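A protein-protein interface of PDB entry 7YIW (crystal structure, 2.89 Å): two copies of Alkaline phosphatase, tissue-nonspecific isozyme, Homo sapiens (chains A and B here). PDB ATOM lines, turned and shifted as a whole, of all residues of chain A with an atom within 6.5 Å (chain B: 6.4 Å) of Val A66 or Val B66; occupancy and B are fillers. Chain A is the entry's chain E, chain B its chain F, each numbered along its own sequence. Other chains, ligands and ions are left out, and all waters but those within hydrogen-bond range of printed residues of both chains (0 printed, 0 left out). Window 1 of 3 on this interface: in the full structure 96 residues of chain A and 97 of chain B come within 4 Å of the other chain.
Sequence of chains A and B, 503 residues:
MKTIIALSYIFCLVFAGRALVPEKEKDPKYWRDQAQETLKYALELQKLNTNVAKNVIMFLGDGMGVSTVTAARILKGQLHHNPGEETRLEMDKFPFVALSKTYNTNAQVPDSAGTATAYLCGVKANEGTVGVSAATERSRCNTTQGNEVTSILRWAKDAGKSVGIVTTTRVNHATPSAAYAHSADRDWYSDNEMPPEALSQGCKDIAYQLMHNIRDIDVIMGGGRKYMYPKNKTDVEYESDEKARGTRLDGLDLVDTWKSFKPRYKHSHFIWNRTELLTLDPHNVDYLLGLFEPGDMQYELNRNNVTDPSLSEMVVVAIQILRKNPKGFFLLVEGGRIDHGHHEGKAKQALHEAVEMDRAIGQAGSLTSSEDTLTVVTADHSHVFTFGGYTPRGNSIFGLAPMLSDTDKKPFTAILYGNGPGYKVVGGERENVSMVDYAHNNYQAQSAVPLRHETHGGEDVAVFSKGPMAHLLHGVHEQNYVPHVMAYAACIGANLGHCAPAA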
ATOM      1  N   MET A  64      -9.714 -24.123 -27.864  1.00  0.00           N
ATOM      2  CA  MET A  64     -10.048 -22.744 -27.513  1.00  0.00           C
ATOM      3  C   MET A  64      -9.000 -22.258 -26.515  1.00  0.00           C
ATOM      4  O   MET A  64      -9.137 -22.412 -25.300  1.00  0.00           O
ATOM      5  CB  MET A  64     -11.474 -22.666 -26.977  1.00  0.00           C
ATOM      6  CG  MET A  64     -11.834 -21.404 -26.213  1.00  0.00           C
ATOM      7  SD  MET A  64     -13.369 -21.609 -25.290  1.00  0.00           S
ATOM      8  CE  MET A  64     -12.728 -22.029 -23.670  1.00  0.00           C
ATOM      9  N   GLY A  65      -7.920 -21.681 -27.043  1.00  0.00           N
ATOM     10  CA  GLY A  65      -6.842 -21.176 -26.220  1.00  0.00           C
ATOM     11  C   GLY A  65      -7.089 -19.754 -25.749  1.00  0.00           C
ATOM     12  O   GLY A  65      -8.117 -19.143 -26.030  1.00  0.00           O
ATOM     13  N   VAL A  66      -6.098 -19.220 -25.026  1.00  0.00           N
ATOM     14  CA  VAL A  66      -6.246 -17.912 -24.388  1.00  0.00           C
ATOM     15  C   VAL A  66      -6.560 -16.835 -25.422  1.00  0.00           C
ATOM     16  O   VAL A  66      -7.429 -15.982 -25.205  1.00  0.00           O
ATOM     17  CB  VAL A  66      -4.983 -17.570 -23.572  1.00  0.00           C
ATOM     18  CG1 VAL A  66      -4.708 -16.071 -23.589  1.00  0.00           C
ATOM     19  CG2 VAL A  66      -5.127 -18.064 -22.142  1.00  0.00           C
ATOM     20  N   SER A  67      -5.870 -16.863 -26.567  1.00  0.00           N
ATOM     21  CA  SER A  67      -6.128 -15.874 -27.607  1.00  0.00           C
ATOM     22  C   SER A  67      -7.456 -16.109 -28.315  1.00  0.00           C
ATOM     23  O   SER A  67      -8.012 -15.168 -28.890  1.00  0.00           O
ATOM     24  CB  SER A  67      -4.985 -15.856 -28.626  1.00  0.00           C
ATOM     25  OG  SER A  67      -4.871 -17.094 -29.303  1.00  0.00           O
ATOM     26  N   THR A  68      -7.978 -17.339 -28.284  1.00  0.00           N
ATOM     27  CA  THR A  68      -9.284 -17.598 -28.879  1.00  0.00           C
ATOM     28  C   THR A  68     -10.406 -17.019 -28.021  1.00  0.00           C
ATOM     29  O   THR A  68     -11.374 -16.463 -28.553  1.00  0.00           O
ATOM     30  CB  THR A  68      -9.482 -19.103 -29.083  1.00  0.00           C
ATOM     31  OG1 THR A  68      -8.516 -19.592 -30.022  1.00  0.00           O
ATOM     32  CG2 THR A  68     -10.880 -19.400 -29.608  1.00  0.00           C
ATOM     33  N   VAL A  69     -10.286 -17.123 -26.692  1.00  0.00           N
ATOM     34  CA  VAL A  69     -11.371 -16.673 -25.823  1.00  0.00           C
ATOM     35  C   VAL A  69     -11.506 -15.155 -25.851  1.00  0.00           C
ATOM     36  O   VAL A  69     -12.615 -14.625 -25.718  1.00  0.00           O
ATOM     37  CB  VAL A  69     -11.183 -17.198 -24.382  1.00  0.00           C
ATOM     38  CG1 VAL A  69     -10.680 -18.625 -24.391  1.00  0.00           C
ATOM     39  CG2 VAL A  69     -10.245 -16.308 -23.571  1.00  0.00           C
ATOM     40  N   THR A  70     -10.401 -14.428 -26.035  1.00  0.00           N
ATOM     41  CA  THR A  70     -10.488 -12.972 -26.071  1.00  0.00           C
ATOM     42  C   THR A  70     -11.112 -12.500 -27.377  1.00  0.00           C
ATOM     43  O   THR A  70     -12.001 -11.639 -27.376  1.00  0.00           O
ATOM     44  CB  THR A  70      -9.106 -12.350 -25.874  1.00  0.00           C
ATOM     45  OG1 THR A  70      -8.582 -12.748 -24.601  1.00  0.00           O
ATOM     46  CG2 THR A  70      -9.197 -10.833 -25.924  1.00  0.00           C
ATOM     47  N   ALA A  71     -10.664 -13.063 -28.502  1.00  0.00           N
ATOM     48  CA  ALA A  71     -11.274 -12.737 -29.787  1.00  0.00           C
ATOM     49  C   ALA A  71     -12.760 -13.076 -29.793  1.00  0.00           C
ATOM     50  O   ALA A  71     -13.567 -12.350 -30.386  1.00  0.00           O
ATOM     51  CB  ALA A  71     -10.548 -13.473 -30.913  1.00  0.00           C
ATOM     52  N   ARG A  73     -14.647 -13.092 -27.046  1.00  0.00           N
ATOM     53  CA  ARG A  73     -15.240 -12.077 -26.181  1.00  0.00           C
ATOM     54  C   ARG A  73     -15.562 -10.811 -26.964  1.00  0.00           C
ATOM     55  O   ARG A  73     -16.624 -10.208 -26.776  1.00  0.00           O
ATOM     56  CB  ARG A  73     -14.293 -11.766 -25.022  1.00  0.00           C
ATOM     57  CG  ARG A  73     -14.785 -10.698 -24.060  1.00  0.00           C
ATOM     58  CD  ARG A  73     -13.648 -10.225 -23.173  1.00  0.00           C
ATOM     59  NE  ARG A  73     -12.996 -11.339 -22.494  1.00  0.00           N
ATOM     60  CZ  ARG A  73     -11.682 -11.496 -22.403  1.00  0.00           C
ATOM     61  NH1 ARG A  73     -10.843 -10.621 -22.935  1.00  0.00           N
ATOM     62  NH2 ARG A  73     -11.198 -12.557 -21.766  1.00  0.00           N
ATOM     63  N   LEU A  99      -4.261 -22.098 -15.075  1.00  0.00           N
ATOM     64  CA  LEU A  99      -3.593 -22.394 -16.334  1.00  0.00           C
ATOM     65  C   LEU A  99      -3.202 -23.865 -16.371  1.00  0.00           C
ATOM     66  O   LEU A  99      -2.702 -24.410 -15.382  1.00  0.00           O
ATOM     67  CB  LEU A  99      -2.357 -21.507 -16.533  1.00  0.00           C
ATOM     68  CG  LEU A  99      -2.647 -20.039 -16.856  1.00  0.00           C
ATOM     69  CD1 LEU A  99      -1.356 -19.262 -17.060  1.00  0.00           C
ATOM     70  CD2 LEU A  99      -3.547 -19.923 -18.079  1.00  0.00           C
ATOM     71  N   SER A 382      -4.263 -25.425 -27.645  1.00  0.00           N
ATOM     72  CA  SER A 382      -4.469 -24.153 -28.320  1.00  0.00           C
ATOM     73  C   SER A 382      -4.145 -24.281 -29.809  1.00  0.00           C
ATOM     74  O   SER A 382      -3.939 -25.377 -30.334  1.00  0.00           O
ATOM     75  CB  SER A 382      -3.626 -23.062 -27.657  1.00  0.00           C
ATOM     76  OG  SER A 382      -4.188 -21.781 -27.872  1.00  0.00           O
ATOM     77  N   GLU A 459       1.216 -23.534 -26.108  1.00  0.00           N
ATOM     78  CA  GLU A 459       0.978 -22.664 -24.967  1.00  0.00           C
ATOM     79  C   GLU A 459      -0.025 -23.294 -24.006  1.00  0.00           C
ATOM     80  O   GLU A 459      -0.769 -24.216 -24.352  1.00  0.00           O
ATOM     81  CB  GLU A 459       0.451 -21.308 -25.436  1.00  0.00           C
ATOM     82  CG  GLU A 459      -0.905 -21.402 -26.111  1.00  0.00           C
ATOM     83  CD  GLU A 459      -1.035 -20.510 -27.328  1.00  0.00           C
ATOM     84  OE1 GLU A 459      -0.492 -20.878 -28.391  1.00  0.00           O
ATOM     85  OE2 GLU A 459      -1.697 -19.455 -27.230  1.00  0.00           O
ATOM     86  N   ASP A 460      -0.043 -22.773 -22.781  1.00  0.00           N
ATOM     87  CA  ASP A 460      -1.037 -23.193 -21.808  1.00  0.00           C
ATOM     88  C   ASP A 460      -2.424 -22.711 -22.225  1.00  0.00           C
ATOM     89  O   ASP A 460      -2.578 -21.794 -23.039  1.00  0.00           O
ATOM     90  CB  ASP A 460      -0.699 -22.653 -20.417  1.00  0.00           C
ATOM     91  CG  ASP A 460       0.671 -23.097 -19.932  1.00  0.00           C
ATOM     92  OD1 ASP A 460       1.205 -24.089 -20.472  1.00  0.00           O
ATOM     93  OD2 ASP A 460       1.213 -22.450 -19.010  1.00  0.00           O
ATOM     94  N   VAL A 461      -3.444 -23.350 -21.659  1.00  0.00           N
ATOM     95  CA  VAL A 461      -4.825 -22.947 -21.877  1.00  0.00           C
ATOM     96  C   VAL A 461      -5.441 -22.589 -20.532  1.00  0.00           C
ATOM     97  O   VAL A 461      -4.916 -22.924 -19.467  1.00  0.00           O
ATOM     98  CB  VAL A 461      -5.657 -24.035 -22.584  1.00  0.00           C
ATOM     99  CG1 VAL A 461      -5.208 -24.186 -24.025  1.00  0.00           C
ATOM    100  CG2 VAL A 461      -5.555 -25.351 -21.840  1.00  0.00           C
ATOM    101  N   ALA A 462      -6.573 -21.900 -20.593  1.00  0.00           N
ATOM    102  CA  ALA A 462      -7.224 -21.380 -19.402  1.00  0.00           C
ATOM    103  C   ALA A 462      -8.223 -22.381 -18.839  1.00  0.00           C
ATOM    104  O   ALA A 462      -8.884 -23.117 -19.577  1.00  0.00           O
ATOM    105  CB  ALA A 462      -7.936 -20.062 -19.710  1.00  0.00           C
ATOM    106  N   MET B  64       4.963 -10.206 -22.038  1.00  0.00           N
ATOM    107  CA  MET B  64       5.089 -11.597 -21.604  1.00  0.00           C
ATOM    108  C   MET B  64       3.706 -12.245 -21.578  1.00  0.00           C
ATOM    109  O   MET B  64       3.072 -12.410 -20.533  1.00  0.00           O
ATOM    110  CB  MET B  64       5.769 -11.660 -20.241  1.00  0.00           C
ATOM    111  CG  MET B  64       6.625 -12.892 -20.013  1.00  0.00           C
ATOM    112  SD  MET B  64       6.847 -13.239 -18.258  1.00  0.00           S
ATOM    113  CE  MET B  64       5.151 -13.174 -17.688  1.00  0.00           C
ATOM    114  N   GLY B  65       3.241 -12.633 -22.765  1.00  0.00           N
ATOM    115  CA  GLY B  65       1.961 -13.292 -22.903  1.00  0.00           C
ATOM    116  C   GLY B  65       2.006 -14.753 -22.493  1.00  0.00           C
ATOM    117  O   GLY B  65       3.035 -15.289 -22.081  1.00  0.00           O
ATOM    118  N   VAL B  66       0.850 -15.409 -22.621  1.00  0.00           N
ATOM    119  CA  VAL B  66       0.731 -16.802 -22.198  1.00  0.00           C
ATOM    120  C   VAL B  66       1.617 -17.702 -23.050  1.00  0.00           C
ATOM    121  O   VAL B  66       2.231 -18.651 -22.543  1.00  0.00           O
ATOM    122  CB  VAL B  66      -0.744 -17.245 -22.243  1.00  0.00           C
ATOM    123  CG1 VAL B  66      -0.867 -18.742 -22.005  1.00  0.00           C
ATOM    124  CG2 VAL B  66      -1.555 -16.479 -21.212  1.00  0.00           C
ATOM    125  N   SER B  67       1.708 -17.422 -24.352  1.00  0.00           N
ATOM    126  CA  SER B  67       2.579 -18.214 -25.213  1.00  0.00           C
ATOM    127  C   SER B  67       4.047 -18.013 -24.861  1.00  0.00           C
ATOM    128  O   SER B  67       4.856 -18.933 -25.028  1.00  0.00           O
ATOM    129  CB  SER B  67       2.333 -17.860 -26.680  1.00  0.00           C
ATOM    130  OG  SER B  67       2.364 -16.458 -26.887  1.00  0.00           O
ATOM    131  N   THR B  68       4.406 -16.827 -24.365  1.00  0.00           N
ATOM    132  CA  THR B  68       5.796 -16.563 -24.014  1.00  0.00           C
ATOM    133  C   THR B  68       6.205 -17.316 -22.753  1.00  0.00           C
ATOM    134  O   THR B  68       7.306 -17.877 -22.691  1.00  0.00           O
ATOM    135  CB  THR B  68       6.015 -15.058 -23.840  1.00  0.00           C
ATOM    136  OG1 THR B  68       6.004 -14.422 -25.125  1.00  0.00           O
ATOM    137  CG2 THR B  68       7.345 -14.780 -23.155  1.00  0.00           C
ATOM    138  N   VAL B  69       5.332 -17.353 -21.742  1.00  0.00           N
ATOM    139  CA  VAL B  69       5.696 -18.010 -20.488  1.00  0.00           C
ATOM    140  C   VAL B  69       5.884 -19.511 -20.686  1.00  0.00           C
ATOM    141  O   VAL B  69       6.735 -20.123 -20.032  1.00  0.00           O
ATOM    142  CB  VAL B  69       4.660 -17.706 -19.383  1.00  0.00           C
ATOM    143  CG1 VAL B  69       4.276 -16.240 -19.395  1.00  0.00           C
ATOM    144  CG2 VAL B  69       3.420 -18.588 -19.513  1.00  0.00           C
ATOM    145  N   THR B  70       5.120 -20.127 -21.593  1.00  0.00           N
ATOM    146  CA  THR B  70       5.269 -21.561 -21.813  1.00  0.00           C
ATOM    147  C   THR B  70       6.562 -21.870 -22.554  1.00  0.00           C
ATOM    148  O   THR B  70       7.280 -22.811 -22.200  1.00  0.00           O
ATOM    149  CB  THR B  70       4.062 -22.108 -22.579  1.00  0.00           C
ATOM    150  OG1 THR B  70       2.857 -21.773 -21.880  1.00  0.00           O
ATOM    151  CG2 THR B  70       4.154 -23.625 -22.713  1.00  0.00           C
ATOM    152  N   ALA B  71       6.881 -21.079 -23.582  1.00  0.00           N
ATOM    153  CA  ALA B  71       8.137 -21.265 -24.297  1.00  0.00           C
ATOM    154  C   ALA B  71       9.333 -20.959 -23.404  1.00  0.00           C
ATOM    155  O   ALA B  71      10.358 -21.647 -23.474  1.00  0.00           O
ATOM    156  CB  ALA B  71       8.160 -20.390 -25.550  1.00  0.00           C
ATOM    157  N   LEU B  99      -6.410 -13.835 -15.192  1.00  0.00           N
ATOM    158  CA  LEU B  99      -6.262 -13.318 -16.546  1.00  0.00           C
ATOM    159  C   LEU B  99      -6.569 -11.827 -16.555  1.00  0.00           C
ATOM    160  O   LEU B  99      -7.485 -11.369 -15.863  1.00  0.00           O
ATOM    161  CB  LEU B  99      -7.185 -14.050 -17.529  1.00  0.00           C
ATOM    162  CG  LEU B  99      -6.873 -15.519 -17.823  1.00  0.00           C
ATOM    163  CD1 LEU B  99      -7.869 -16.088 -18.820  1.00  0.00           C
ATOM    164  CD2 LEU B  99      -5.450 -15.682 -18.332  1.00  0.00           C
ATOM    165  N   SER B 382       0.384  -8.734 -24.832  1.00  0.00           N
ATOM    166  CA  SER B 382       1.045  -9.896 -25.392  1.00  0.00           C
ATOM    167  C   SER B 382       1.708  -9.541 -26.725  1.00  0.00           C
ATOM    168  O   SER B 382       1.931  -8.362 -27.028  1.00  0.00           O
ATOM    169  CB  SER B 382       0.029 -11.031 -25.527  1.00  0.00           C
ATOM    170  OG  SER B 382       0.672 -12.244 -25.863  1.00  0.00           O
ATOM    171  N   PHE B 387       4.041 -20.871 -31.175  1.00  0.00           N
ATOM    172  CA  PHE B 387       4.956 -21.965 -31.448  1.00  0.00           C
ATOM    173  C   PHE B 387       4.153 -23.255 -31.504  1.00  0.00           C
ATOM    174  O   PHE B 387       3.168 -23.422 -30.781  1.00  0.00           O
ATOM    175  CB  PHE B 387       6.083 -22.057 -30.409  1.00  0.00           C
ATOM    176  CG  PHE B 387       5.666 -22.661 -29.101  1.00  0.00           C
ATOM    177  CD1 PHE B 387       4.965 -21.915 -28.168  1.00  0.00           C
ATOM    178  CD2 PHE B 387       5.992 -23.973 -28.797  1.00  0.00           C
ATOM    179  CE1 PHE B 387       4.588 -22.471 -26.960  1.00  0.00           C
ATOM    180  CE2 PHE B 387       5.619 -24.533 -27.593  1.00  0.00           C
ATOM    181  CZ  PHE B 387       4.918 -23.782 -26.673  1.00  0.00           C
ATOM    182  N   GLU B 459      -4.765 -10.363 -27.023  1.00  0.00           N
ATOM    183  CA  GLU B 459      -5.256 -11.397 -26.128  1.00  0.00           C
ATOM    184  C   GLU B 459      -4.822 -11.119 -24.691  1.00  0.00           C
ATOM    185  O   GLU B 459      -3.911 -10.329 -24.426  1.00  0.00           O
ATOM    186  CB  GLU B 459      -4.768 -12.776 -26.574  1.00  0.00           C
ATOM    187  CG  GLU B 459      -3.439 -13.208 -25.982  1.00  0.00           C
ATOM    188  CD  GLU B 459      -2.301 -13.099 -26.976  1.00  0.00           C
ATOM    189  OE1 GLU B 459      -2.447 -12.353 -27.968  1.00  0.00           O
ATOM    190  OE2 GLU B 459      -1.263 -13.760 -26.765  1.00  0.00           O
ATOM    191  N   ASP B 460      -5.496 -11.788 -23.757  1.00  0.00           N
ATOM    192  CA  ASP B 460      -5.264 -11.573 -22.337  1.00  0.00           C
ATOM    193  C   ASP B 460      -3.863 -12.037 -21.937  1.00  0.00           C
ATOM    194  O   ASP B 460      -3.163 -12.731 -22.680  1.00  0.00           O
ATOM    195  CB  ASP B 460      -6.315 -12.309 -21.507  1.00  0.00           C
ATOM    196  CG  ASP B 460      -7.723 -11.826 -21.787  1.00  0.00           C
ATOM    197  OD1 ASP B 460      -7.873 -10.719 -22.347  1.00  0.00           O
ATOM    198  OD2 ASP B 460      -8.680 -12.554 -21.449  1.00  0.00           O
ATOM    199  N   VAL B 461      -3.457 -11.636 -20.730  1.00  0.00           N
ATOM    200  CA  VAL B 461      -2.191 -12.050 -20.143  1.00  0.00           C
ATOM    201  C   VAL B 461      -2.469 -12.659 -18.775  1.00  0.00           C
ATOM    202  O   VAL B 461      -3.546 -12.491 -18.200  1.00  0.00           O
ATOM    203  CB  VAL B 461      -1.185 -10.884 -20.022  1.00  0.00           C
ATOM    204  CG1 VAL B 461      -0.833 -10.342 -21.396  1.00  0.00           C
ATOM    205  CG2 VAL B 461      -1.746  -9.783 -19.135  1.00  0.00           C
ATOM    206  N   ALA B 462      -1.475 -13.373 -18.257  1.00  0.00           N
ATOM    207  CA  ALA B 462      -1.605 -14.058 -16.980  1.00  0.00           C
ATOM    208  C   ALA B 462      -1.147 -13.161 -15.837  1.00  0.00           C
ATOM    209  O   ALA B 462      -0.302 -12.277 -16.011  1.00  0.00           O
ATOM    210  CB  ALA B 462      -0.797 -15.356 -16.978  1.00  0.00           C
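Of the 15 printed residues of chain A, 7 touch a printed residue of chain B.
Hydrophobic or aromatic side chains of chain A within 4 Å of the printed part of chain B: Val A66 and Leu A99.
Val B66 touches just these residues of chain A: Val A66 and Asp A460.
Of the printed residues of chain A, Thr B70 touches Glu A459 (3.7 Å) and Asp A460 (3.2 Å).
Printed residues of chain B within 4 Å of Glu A459: Ser B67 (3.8 Å), Thr B70 (3.7 Å) and Phe B387 (3.6 Å).
Of the printed residues of chain A, Asp B460 touches Val A66, Thr A70 and Arg A73.
Of the printed residues of chain A, Glu B459 touches Val A66, Ser A67 and Thr A70.
Of the printed residues of chain A, Ser B67 touches Glu A459 (3.8 Å).
Leu B99 touches none of the printed residues of chain A.
The nearest residue of chain A that does not touch Val B66 is Glu A459 (4.3 Å).
The nearest printed residue of chain B that does not touch Asp A460 is Val B69 (4.5 Å).
Val A66 touches its own counterpart, Val B66.
Val A66 touches Asp B460, and with the chains exchanged Asp A460 touches Val B66.
Ser A67 touches Glu B459, and with the chains exchanged Glu A459 touches Ser B67.
Thr A70 touches Glu B459, and with the chains exchanged Glu A459 touches Thr B70.
14 positions are printed for both chains.
Of the 13 pairs that touch across the chains among the printed residues, 9 have their exchanged pair printed and touching as well.
OG1 of Thr A70 lies within hydrogen-bond range of O of Val A66.
OE2 of Glu A459 lies close to OG of Ser A382, at 3.5 Å.
The backbone carbonyl oxygen (O) of Val B66 is in hydrogen-bond range of the side-chain hydroxyl (OG1) of Thr B70 (3.3 Å).
The side-chain carboxylate of Glu B459 lies within hydrogen-bond range of the side-chain hydroxyl of Ser B382, 2.6 Å away.
OD1 of Asp B460 sits close to OG1 of Thr A70, 3.1 Å away.
The side-chain carboxylate (OD1) of Asp A460 is in hydrogen-bond range of the side-chain hydroxyl (OG1) of Thr B70, 3.2 Å away.
The guanidinium group (NH2) of Arg A73 lies within salt-bridge range of the side-chain carboxylate (OD2) of Asp B460 (2.5 Å).
CG2 of Val B66 touches CG1 of Val A66, at 3.97 Å.
CG1 of Val A66 touches CG of Glu B459 (3.9 Å).
Asp B460 touches Val A66 (O to CG1, 3.8 Å).
CA of Ser A67 touches CB of Glu B459, at 3.5 Å.
Thr A70 touches Glu B459 (OG1 to CA, 3.9 Å).
Ala B462 touches Leu A99 (CB to CD1, 3.9 Å).
Ser B67 touches Glu A459.
Glu A459 touches Thr B70.
N of Glu A459 touches CE1 of Phe B387 (3.6 Å).
Asp A460 touches Val B66 (O to CG1, 3.6 Å).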
